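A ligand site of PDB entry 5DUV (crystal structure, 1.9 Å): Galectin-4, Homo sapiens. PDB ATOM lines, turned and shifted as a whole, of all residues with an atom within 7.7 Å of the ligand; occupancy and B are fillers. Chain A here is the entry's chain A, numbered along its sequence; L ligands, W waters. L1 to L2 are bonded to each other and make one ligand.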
ATOM      1  N   ARG A  45     -34.343 -13.917  32.202  1.00  0.00           N
ATOM      2  CA  ARG A  45     -33.485 -13.054  31.382  1.00  0.00           C
ATOM      3  C   ARG A  45     -34.065 -11.650  31.335  1.00  0.00           C
ATOM      4  O   ARG A  45     -35.261 -11.452  31.534  1.00  0.00           O
ATOM      5  CB  ARG A  45     -33.401 -13.561  29.945  1.00  0.00           C
ATOM      6  CG  ARG A  45     -32.866 -14.975  29.782  1.00  0.00           C
ATOM      7  CD  ARG A  45     -32.593 -15.319  28.329  1.00  0.00           C
ATOM      8  NE  ARG A  45     -31.972 -16.636  28.211  1.00  0.00           N
ATOM      9  CZ  ARG A  45     -31.629 -17.215  27.063  1.00  0.00           C
ATOM     10  NH1 ARG A  45     -31.860 -16.601  25.902  1.00  0.00           N
ATOM     11  NH2 ARG A  45     -31.075 -18.431  27.072  1.00  0.00           N
ATOM     12  N   PHE A  46     -33.203 -10.684  31.036  1.00  0.00           N
ATOM     13  CA  PHE A  46     -33.646  -9.457  30.420  1.00  0.00           C
ATOM     14  C   PHE A  46     -32.558  -8.972  29.462  1.00  0.00           C
ATOM     15  O   PHE A  46     -31.453  -9.505  29.440  1.00  0.00           O
ATOM     16  CB  PHE A  46     -34.106  -8.400  31.444  1.00  0.00           C
ATOM     17  CG  PHE A  46     -33.007  -7.750  32.257  1.00  0.00           C
ATOM     18  CD1 PHE A  46     -32.229  -6.726  31.731  1.00  0.00           C
ATOM     19  CD2 PHE A  46     -32.843  -8.086  33.589  1.00  0.00           C
ATOM     20  CE1 PHE A  46     -31.265  -6.095  32.497  1.00  0.00           C
ATOM     21  CE2 PHE A  46     -31.884  -7.453  34.375  1.00  0.00           C
ATOM     22  CZ  PHE A  46     -31.096  -6.453  33.822  1.00  0.00           C
ATOM     23  N   PHE A  47     -32.913  -8.032  28.598  1.00  0.00           N
ATOM     24  CA  PHE A  47     -31.915  -7.478  27.692  1.00  0.00           C
ATOM     25  C   PHE A  47     -32.039  -5.981  27.595  1.00  0.00           C
ATOM     26  O   PHE A  47     -33.112  -5.419  27.833  1.00  0.00           O
ATOM     27  CB  PHE A  47     -31.953  -8.133  26.310  1.00  0.00           C
ATOM     28  CG  PHE A  47     -33.183  -7.828  25.508  1.00  0.00           C
ATOM     29  CD1 PHE A  47     -33.374  -6.584  24.949  1.00  0.00           C
ATOM     30  CD2 PHE A  47     -34.126  -8.812  25.285  1.00  0.00           C
ATOM     31  CE1 PHE A  47     -34.512  -6.308  24.197  1.00  0.00           C
ATOM     32  CE2 PHE A  47     -35.268  -8.556  24.554  1.00  0.00           C
ATOM     33  CZ  PHE A  47     -35.458  -7.298  24.005  1.00  0.00           C
ATOM     34  N   ASN A  49     -30.919  -3.387  24.529  1.00  0.00           N
ATOM     35  CA  ASN A  49     -30.408  -3.300  23.170  1.00  0.00           C
ATOM     36  C   ASN A  49     -30.202  -1.861  22.765  1.00  0.00           C
ATOM     37  O   ASN A  49     -31.065  -1.026  22.959  1.00  0.00           O
ATOM     38  CB  ASN A  49     -31.404  -3.901  22.183  1.00  0.00           C
ATOM     39  CG  ASN A  49     -31.379  -5.412  22.170  1.00  0.00           C
ATOM     40  OD1 ASN A  49     -30.427  -6.037  22.625  1.00  0.00           O
ATOM     41  ND2 ASN A  49     -32.438  -6.005  21.624  1.00  0.00           N
ATOM     42  N   HIS A  63     -26.239  -5.771  22.210  1.00  0.00           N
ATOM     43  CA  HIS A  63     -27.213  -6.555  22.949  1.00  0.00           C
ATOM     44  C   HIS A  63     -26.562  -7.009  24.262  1.00  0.00           C
ATOM     45  O   HIS A  63     -25.535  -7.712  24.256  1.00  0.00           O
ATOM     46  CB  HIS A  63     -27.617  -7.758  22.074  1.00  0.00           C
ATOM     47  CG  HIS A  63     -28.435  -8.811  22.759  1.00  0.00           C
ATOM     48  ND1 HIS A  63     -29.783  -8.667  23.036  1.00  0.00           N
ATOM     49  CD2 HIS A  63     -28.125 -10.084  23.124  1.00  0.00           C
ATOM     50  CE1 HIS A  63     -30.244  -9.765  23.585  1.00  0.00           C
ATOM     51  NE2 HIS A  63     -29.255 -10.645  23.661  1.00  0.00           N
ATOM     52  N   PHE A  64     -27.169  -6.590  25.374  1.00  0.00           N
ATOM     53  CA  PHE A  64     -26.670  -6.887  26.713  1.00  0.00           C
ATOM     54  C   PHE A  64     -27.709  -7.781  27.403  1.00  0.00           C
ATOM     55  O   PHE A  64     -28.825  -7.347  27.652  1.00  0.00           O
ATOM     56  CB  PHE A  64     -26.443  -5.562  27.493  1.00  0.00           C
ATOM     57  CG  PHE A  64     -26.163  -5.747  28.968  1.00  0.00           C
ATOM     58  CD1 PHE A  64     -24.871  -5.941  29.431  1.00  0.00           C
ATOM     59  CD2 PHE A  64     -27.200  -5.728  29.897  1.00  0.00           C
ATOM     60  CE1 PHE A  64     -24.614  -6.124  30.784  1.00  0.00           C
ATOM     61  CE2 PHE A  64     -26.943  -5.896  31.260  1.00  0.00           C
ATOM     62  CZ  PHE A  64     -25.653  -6.097  31.702  1.00  0.00           C
ATOM     63  N   ASN A  65     -27.357  -9.032  27.673  1.00  0.00           N
ATOM     64  CA  ASN A  65     -28.351 -10.051  28.013  1.00  0.00           C
ATOM     65  C   ASN A  65     -27.970 -10.921  29.222  1.00  0.00           C
ATOM     66  O   ASN A  65     -27.425 -12.002  29.048  1.00  0.00           O
ATOM     67  CB  ASN A  65     -28.557 -10.944  26.765  1.00  0.00           C
ATOM     68  CG  ASN A  65     -29.694 -11.954  26.908  1.00  0.00           C
ATOM     69  OD1 ASN A  65     -29.624 -13.042  26.342  1.00  0.00           O
ATOM     70  ND2 ASN A  65     -30.730 -11.620  27.639  1.00  0.00           N
ATOM     71  N   ARG A  67     -28.570 -13.625  32.090  1.00  0.00           N
ATOM     72  CA  ARG A  67     -29.301 -14.886  32.018  1.00  0.00           C
ATOM     73  C   ARG A  67     -29.057 -15.719  33.257  1.00  0.00           C
ATOM     74  O   ARG A  67     -27.903 -15.953  33.645  1.00  0.00           O
ATOM     75  CB  ARG A  67     -28.829 -15.717  30.838  1.00  0.00           C
ATOM     76  CG  ARG A  67     -28.872 -15.064  29.464  1.00  0.00           C
ATOM     77  CD  ARG A  67     -28.468 -16.079  28.409  1.00  0.00           C
ATOM     78  NE  ARG A  67     -28.530 -15.558  27.065  1.00  0.00           N
ATOM     79  CZ  ARG A  67     -28.143 -16.233  25.991  1.00  0.00           C
ATOM     80  NH1 ARG A  67     -27.649 -17.467  26.111  1.00  0.00           N
ATOM     81  NH2 ARG A  67     -28.249 -15.674  24.798  1.00  0.00           N
ATOM     82  N   ASP A  69     -30.591 -18.839  33.238  1.00  0.00           N
ATOM     83  CA  ASP A  69     -30.659 -20.210  32.746  1.00  0.00           C
ATOM     84  C   ASP A  69     -29.241 -20.763  32.604  1.00  0.00           C
ATOM     85  O   ASP A  69     -28.355 -20.125  32.033  1.00  0.00           O
ATOM     86  CB  ASP A  69     -31.441 -20.329  31.424  1.00  0.00           C
ATOM     87  CG  ASP A  69     -30.966 -19.361  30.350  1.00  0.00           C
ATOM     88  OD1 ASP A  69     -31.245 -18.153  30.480  1.00  0.00           O
ATOM     89  OD2 ASP A  69     -30.324 -19.821  29.366  1.00  0.00           O
ATOM     90  N   LYS A  73     -24.948 -15.927  34.037  1.00  0.00           N
ATOM     91  CA  LYS A  73     -24.001 -15.294  33.140  1.00  0.00           C
ATOM     92  C   LYS A  73     -24.603 -14.094  32.451  1.00  0.00           C
ATOM     93  O   LYS A  73     -25.797 -13.819  32.580  1.00  0.00           O
ATOM     94  CB  LYS A  73     -23.517 -16.307  32.097  1.00  0.00           C
ATOM     95  CG  LYS A  73     -24.587 -16.771  31.117  1.00  0.00           C
ATOM     96  CD  LYS A  73     -24.022 -17.860  30.198  1.00  0.00           C
ATOM     97  CE  LYS A  73     -25.058 -18.884  29.797  1.00  0.00           C
ATOM     98  NZ  LYS A  73     -25.543 -19.739  30.919  1.00  0.00           N
ATOM     99  N   VAL A  75     -24.497 -12.299  28.496  1.00  0.00           N
ATOM    100  CA  VAL A  75     -24.111 -12.501  27.112  1.00  0.00           C
ATOM    101  C   VAL A  75     -24.161 -11.168  26.365  1.00  0.00           C
ATOM    102  O   VAL A  75     -25.029 -10.330  26.630  1.00  0.00           O
ATOM    103  CB  VAL A  75     -25.061 -13.513  26.441  1.00  0.00           C
ATOM    104  CG1 VAL A  75     -24.847 -13.514  24.936  1.00  0.00           C
ATOM    105  CG2 VAL A  75     -24.810 -14.896  27.010  1.00  0.00           C
ATOM    106  N   PHE A  76     -23.202 -10.977  25.465  1.00  0.00           N
ATOM    107  CA  PHE A  76     -23.045  -9.718  24.751  1.00  0.00           C
ATOM    108  C   PHE A  76     -22.869 -10.037  23.289  1.00  0.00           C
ATOM    109  O   PHE A  76     -22.080 -10.909  22.932  1.00  0.00           O
ATOM    110  CB  PHE A  76     -21.808  -8.934  25.192  1.00  0.00           C
ATOM    111  CG  PHE A  76     -21.580  -8.886  26.679  1.00  0.00           C
ATOM    112  CD1 PHE A  76     -22.132  -7.864  27.452  1.00  0.00           C
ATOM    113  CD2 PHE A  76     -20.776  -9.811  27.302  1.00  0.00           C
ATOM    114  CE1 PHE A  76     -21.880  -7.790  28.808  1.00  0.00           C
ATOM    115  CE2 PHE A  76     -20.535  -9.741  28.666  1.00  0.00           C
ATOM    116  CZ  PHE A  76     -21.098  -8.732  29.416  1.00  0.00           C
ATOM    117  N   ASN A  77     -23.558  -9.295  22.436  1.00  0.00           N
ATOM    118  CA  ASN A  77     -23.490  -9.549  21.010  1.00  0.00           C
ATOM    119  C   ASN A  77     -24.066  -8.404  20.189  1.00  0.00           C
ATOM    120  O   ASN A  77     -24.593  -7.403  20.741  1.00  0.00           O
ATOM    121  CB  ASN A  77     -24.207 -10.873  20.667  1.00  0.00           C
ATOM    122  CG  ASN A  77     -23.579 -11.606  19.478  1.00  0.00           C
ATOM    123  OD1 ASN A  77     -22.809 -11.040  18.705  1.00  0.00           O
ATOM    124  ND2 ASN A  77     -23.919 -12.875  19.338  1.00  0.00           N
ATOM    125  N   THR A  78     -23.942  -8.559  18.883  1.00  0.00           N
ATOM    126  CA  THR A  78     -24.400  -7.603  17.894  1.00  0.00           C
ATOM    127  C   THR A  78     -25.204  -8.408  16.888  1.00  0.00           C
ATOM    128  O   THR A  78     -24.820  -9.540  16.550  1.00  0.00           O
ATOM    129  CB  THR A  78     -23.191  -6.907  17.209  1.00  0.00           C
ATOM    130  OG1 THR A  78     -22.556  -6.039  18.151  1.00  0.00           O
ATOM    131  CG2 THR A  78     -23.616  -6.092  15.973  1.00  0.00           C
ATOM    132  N   LEU A  79     -26.314  -7.822  16.445  1.00  0.00           N
ATOM    133  CA  LEU A  79     -27.149  -8.343  15.369  1.00  0.00           C
ATOM    134  C   LEU A  79     -27.001  -7.434  14.148  1.00  0.00           C
ATOM    135  O   LEU A  79     -27.319  -6.255  14.208  1.00  0.00           O
ATOM    136  CB  LEU A  79     -28.620  -8.360  15.796  1.00  0.00           C
ATOM    137  CG  LEU A  79     -29.589  -9.054  14.847  1.00  0.00           C
ATOM    138  CD1 LEU A  79     -29.496 -10.563  15.009  1.00  0.00           C
ATOM    139  CD2 LEU A  79     -31.015  -8.569  15.109  1.00  0.00           C
ATOM    140  N   TRP A  84     -26.800 -12.888  14.291  1.00  0.00           N
ATOM    141  CA  TRP A  84     -25.986 -12.657  15.474  1.00  0.00           C
ATOM    142  C   TRP A  84     -24.523 -12.884  15.123  1.00  0.00           C
ATOM    143  O   TRP A  84     -24.231 -13.781  14.359  1.00  0.00           O
ATOM    144  CB  TRP A  84     -26.395 -13.582  16.615  1.00  0.00           C
ATOM    145  CG  TRP A  84     -27.728 -13.211  17.227  1.00  0.00           C
ATOM    146  CD1 TRP A  84     -28.889 -13.937  17.157  1.00  0.00           C
ATOM    147  CD2 TRP A  84     -28.026 -12.036  17.992  1.00  0.00           C
ATOM    148  NE1 TRP A  84     -29.891 -13.277  17.842  1.00  0.00           N
ATOM    149  CE2 TRP A  84     -29.385 -12.113  18.352  1.00  0.00           C
ATOM    150  CE3 TRP A  84     -27.265 -10.940  18.403  1.00  0.00           C
ATOM    151  CZ2 TRP A  84     -30.014 -11.116  19.106  1.00  0.00           C
ATOM    152  CZ3 TRP A  84     -27.890  -9.944  19.148  1.00  0.00           C
ATOM    153  CH2 TRP A  84     -29.248 -10.037  19.489  1.00  0.00           C
ATOM    154  N   GLY A  85     -23.634 -12.058  15.671  1.00  0.00           N
ATOM    155  CA  GLY A  85     -22.206 -12.271  15.496  1.00  0.00           C
ATOM    156  C   GLY A  85     -21.640 -13.298  16.470  1.00  0.00           C
ATOM    157  O   GLY A  85     -22.396 -14.048  17.099  1.00  0.00           O
ATOM    158  N   SER A  86     -20.322 -13.326  16.610  1.00  0.00           N
ATOM    159  CA  SER A  86     -19.685 -14.152  17.614  1.00  0.00           C
ATOM    160  C   SER A  86     -20.042 -13.607  18.981  1.00  0.00           C
ATOM    161  O   SER A  86     -19.814 -12.443  19.279  1.00  0.00           O
ATOM    162  CB  SER A  86     -18.161 -14.162  17.466  1.00  0.00           C
ATOM    163  OG  SER A  86     -17.810 -14.398  16.118  1.00  0.00           O
ATOM    164  N   GLU A  87     -20.617 -14.477  19.788  1.00  0.00           N
ATOM    165  CA  GLU A  87     -21.033 -14.115  21.126  1.00  0.00           C
ATOM    166  C   GLU A  87     -19.850 -13.856  22.066  1.00  0.00           C
ATOM    167  O   GLU A  87     -18.858 -14.573  22.041  1.00  0.00           O
ATOM    168  CB  GLU A  87     -21.855 -15.274  21.686  1.00  0.00           C
ATOM    169  CG  GLU A  87     -22.947 -14.867  22.633  1.00  0.00           C
ATOM    170  CD  GLU A  87     -23.850 -16.026  22.961  1.00  0.00           C
ATOM    171  OE1 GLU A  87     -25.005 -16.044  22.474  1.00  0.00           O
ATOM    172  OE2 GLU A  87     -23.383 -16.942  23.677  1.00  0.00           O
ATOM    173  N   GLU A  88     -19.971 -12.834  22.896  1.00  0.00           N
ATOM    174  CA  GLU A  88     -19.084 -12.683  24.024  1.00  0.00           C
ATOM    175  C   GLU A  88     -19.852 -13.073  25.280  1.00  0.00           C
ATOM    176  O   GLU A  88     -21.071 -12.910  25.351  1.00  0.00           O
ATOM    177  CB  GLU A  88     -18.549 -11.247  24.107  1.00  0.00           C
ATOM    178  CG  GLU A  88     -17.577 -10.920  22.977  1.00  0.00           C
ATOM    179  CD  GLU A  88     -17.170  -9.457  22.907  1.00  0.00           C
ATOM    180  OE1 GLU A  88     -16.864  -8.823  23.939  1.00  0.00           O
ATOM    181  OE2 GLU A  88     -17.124  -8.935  21.781  1.00  0.00           O
ATOM    182  N   ARG A  89     -19.162 -13.650  26.263  1.00  0.00           N
ATOM    183  CA  ARG A  89     -19.811 -14.034  27.509  1.00  0.00           C
ATOM    184  C   ARG A  89     -18.927 -13.705  28.692  1.00  0.00           C
ATOM    185  O   ARG A  89     -17.703 -13.796  28.614  1.00  0.00           O
ATOM    186  CB  ARG A  89     -20.105 -15.535  27.552  1.00  0.00           C
ATOM    187  CG  ARG A  89     -20.868 -16.078  26.374  1.00  0.00           C
ATOM    188  CD  ARG A  89     -21.203 -17.548  26.579  1.00  0.00           C
ATOM    189  NE  ARG A  89     -22.416 -17.916  25.873  1.00  0.00           N
ATOM    190  CZ  ARG A  89     -23.194 -18.947  26.191  1.00  0.00           C
ATOM    191  NH1 ARG A  89     -22.887 -19.731  27.214  1.00  0.00           N
ATOM    192  NH2 ARG A  89     -24.287 -19.193  25.464  1.00  0.00           N
HETATM  193  C1  LIG L   1     -25.804 -19.614  22.070  1.00  0.00           C
HETATM  194  C2  LIG L   1     -27.001 -18.829  22.573  1.00  0.00           C
HETATM  195  C3  LIG L   1     -27.736 -18.225  21.387  1.00  0.00           C
HETATM  196  C4  LIG L   1     -28.069 -19.326  20.387  1.00  0.00           C
HETATM  197  C5  LIG L   1     -28.768 -18.835  19.139  1.00  0.00           C
HETATM  198  C6  LIG L   1     -26.237 -20.639  21.034  1.00  0.00           C
HETATM  199  O1  LIG L   1     -25.070 -21.305  20.552  1.00  0.00           O
HETATM  200  O2  LIG L   1     -25.223 -20.290  23.179  1.00  0.00           O
HETATM  201  O3  LIG L   1     -26.583 -17.825  23.514  1.00  0.00           O
HETATM  202  O4  LIG L   1     -28.913 -17.591  21.901  1.00  0.00           O
HETATM  203  O5  LIG L   1     -26.872 -19.962  19.952  1.00  0.00           O
HETATM  204  O6  LIG L   1     -27.907 -17.872  18.517  1.00  0.00           O
HETATM  205  C1  LG2 L   2     -29.121 -16.276  21.383  1.00  0.00           C
HETATM  206  C2  LG2 L   2     -30.497 -15.746  21.842  1.00  0.00           C
HETATM  207  C3  LG2 L   2     -30.691 -14.276  21.479  1.00  0.00           C
HETATM  208  C4  LG2 L   2     -29.446 -13.466  21.866  1.00  0.00           C
HETATM  209  C5  LG2 L   2     -28.181 -14.116  21.326  1.00  0.00           C
HETATM  210  C6  LG2 L   2     -26.933 -13.295  21.662  1.00  0.00           C
HETATM  211  O1  LG2 L   2     -31.521 -16.518  21.209  1.00  0.00           O
HETATM  212  O2  LG2 L   2     -31.873 -13.761  22.139  1.00  0.00           O
HETATM  213  O3  LG2 L   2     -29.337 -13.361  23.294  1.00  0.00           O
HETATM  214  O4  LG2 L   2     -28.089 -15.430  21.875  1.00  0.00           O
HETATM  215  O5  LG2 L   2     -25.760 -14.025  21.282  1.00  0.00           O
HETATM  216  O   HOH W   1     -30.323 -18.715  24.046  1.00  0.00           O
HETATM  217  O   HOH W   2     -31.842 -15.889  18.457  1.00  0.00           O
HETATM  218  O   HOH W   3     -25.892 -16.035  19.305  1.00  0.00           O
HETATM  219  O   HOH W   4     -32.943 -11.544  21.621  1.00  0.00           O
HETATM  220  O   HOH W   5     -32.013 -13.832  24.914  1.00  0.00           O
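Merely in contact with the ligand: Trp 84 and Val 75.
Hydrophobic or aromatic side chains within 4 Å of the ligand: His 63, Val 75 and Trp 84.
The side-chain amide oxygen (OD1) of Asn 77 sits close to the backbone carbonyl oxygen (O) of Ser 86, 3.4 Å away.
The guanidinium group (NE) of Arg 89 lies within salt-bridge range of the side-chain carboxylate (OE2) of Glu 87.
ND2 of Asn 65 lies within hydrogen-bond range of O of Phe 46, at 2.9 Å.
O of Gly 85 is in hydrogen-bond range of ND2 of Asn 77 (3.0 Å).
N of Asn 65 is in hydrogen-bond range of O of Val 75, 2.9 Å away.
A ring nitrogen (ND1) of His 63 sits at hydrogen-bond distance from the side-chain amide oxygen of Asn 49 (2.7 Å).
N of Arg 67 sits at hydrogen-bond distance from O of Lys 73, at 2.8 Å.
O of Asn 77 sits at hydrogen-bond distance from N of His 63 (2.7 Å).
An oxygen (O5) of LG2 L2 is in hydrogen-bond range of the side-chain carboxylate (OE1) of Glu 87 (2.5 Å).
NE2 of His 63 is in hydrogen-bond range of O3 of LG2 L2, at 2.7 Å.
The side-chain amide nitrogen (ND2) of Asn 77 lies within hydrogen-bond range of an oxygen (O5) of LG2 L2.
An oxygen (O3) of LG2 L2 is in hydrogen-bond range of the side-chain amide oxygen (OD1) of Asn 65 (3.1 Å).
The guanidinium group (NH1) of Arg 67 sits at hydrogen-bond distance from an oxygen (O3) of LIG L1.
NH2 of Arg 89 is in hydrogen-bond range of O2 of LIG L1.
Water W5 lies within hydrogen-bond range of O2 of LG2 L2 (2.8 Å), OD1 of Asn 65 (2.9 Å) and NH1 of Arg 45 (2.9 Å).
Water W1 bridges O4 of LIG L1 and NH2 of Arg 45.
Water W3 lies within hydrogen-bond range of O5 of LG2 L2 (2.8 Å) and OE1 of Glu 87 (3.3 Å).
Water W2 bridges O1 of LG2 L2 (2.8 Å) and NE1 of Trp 84 (3.3 Å).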
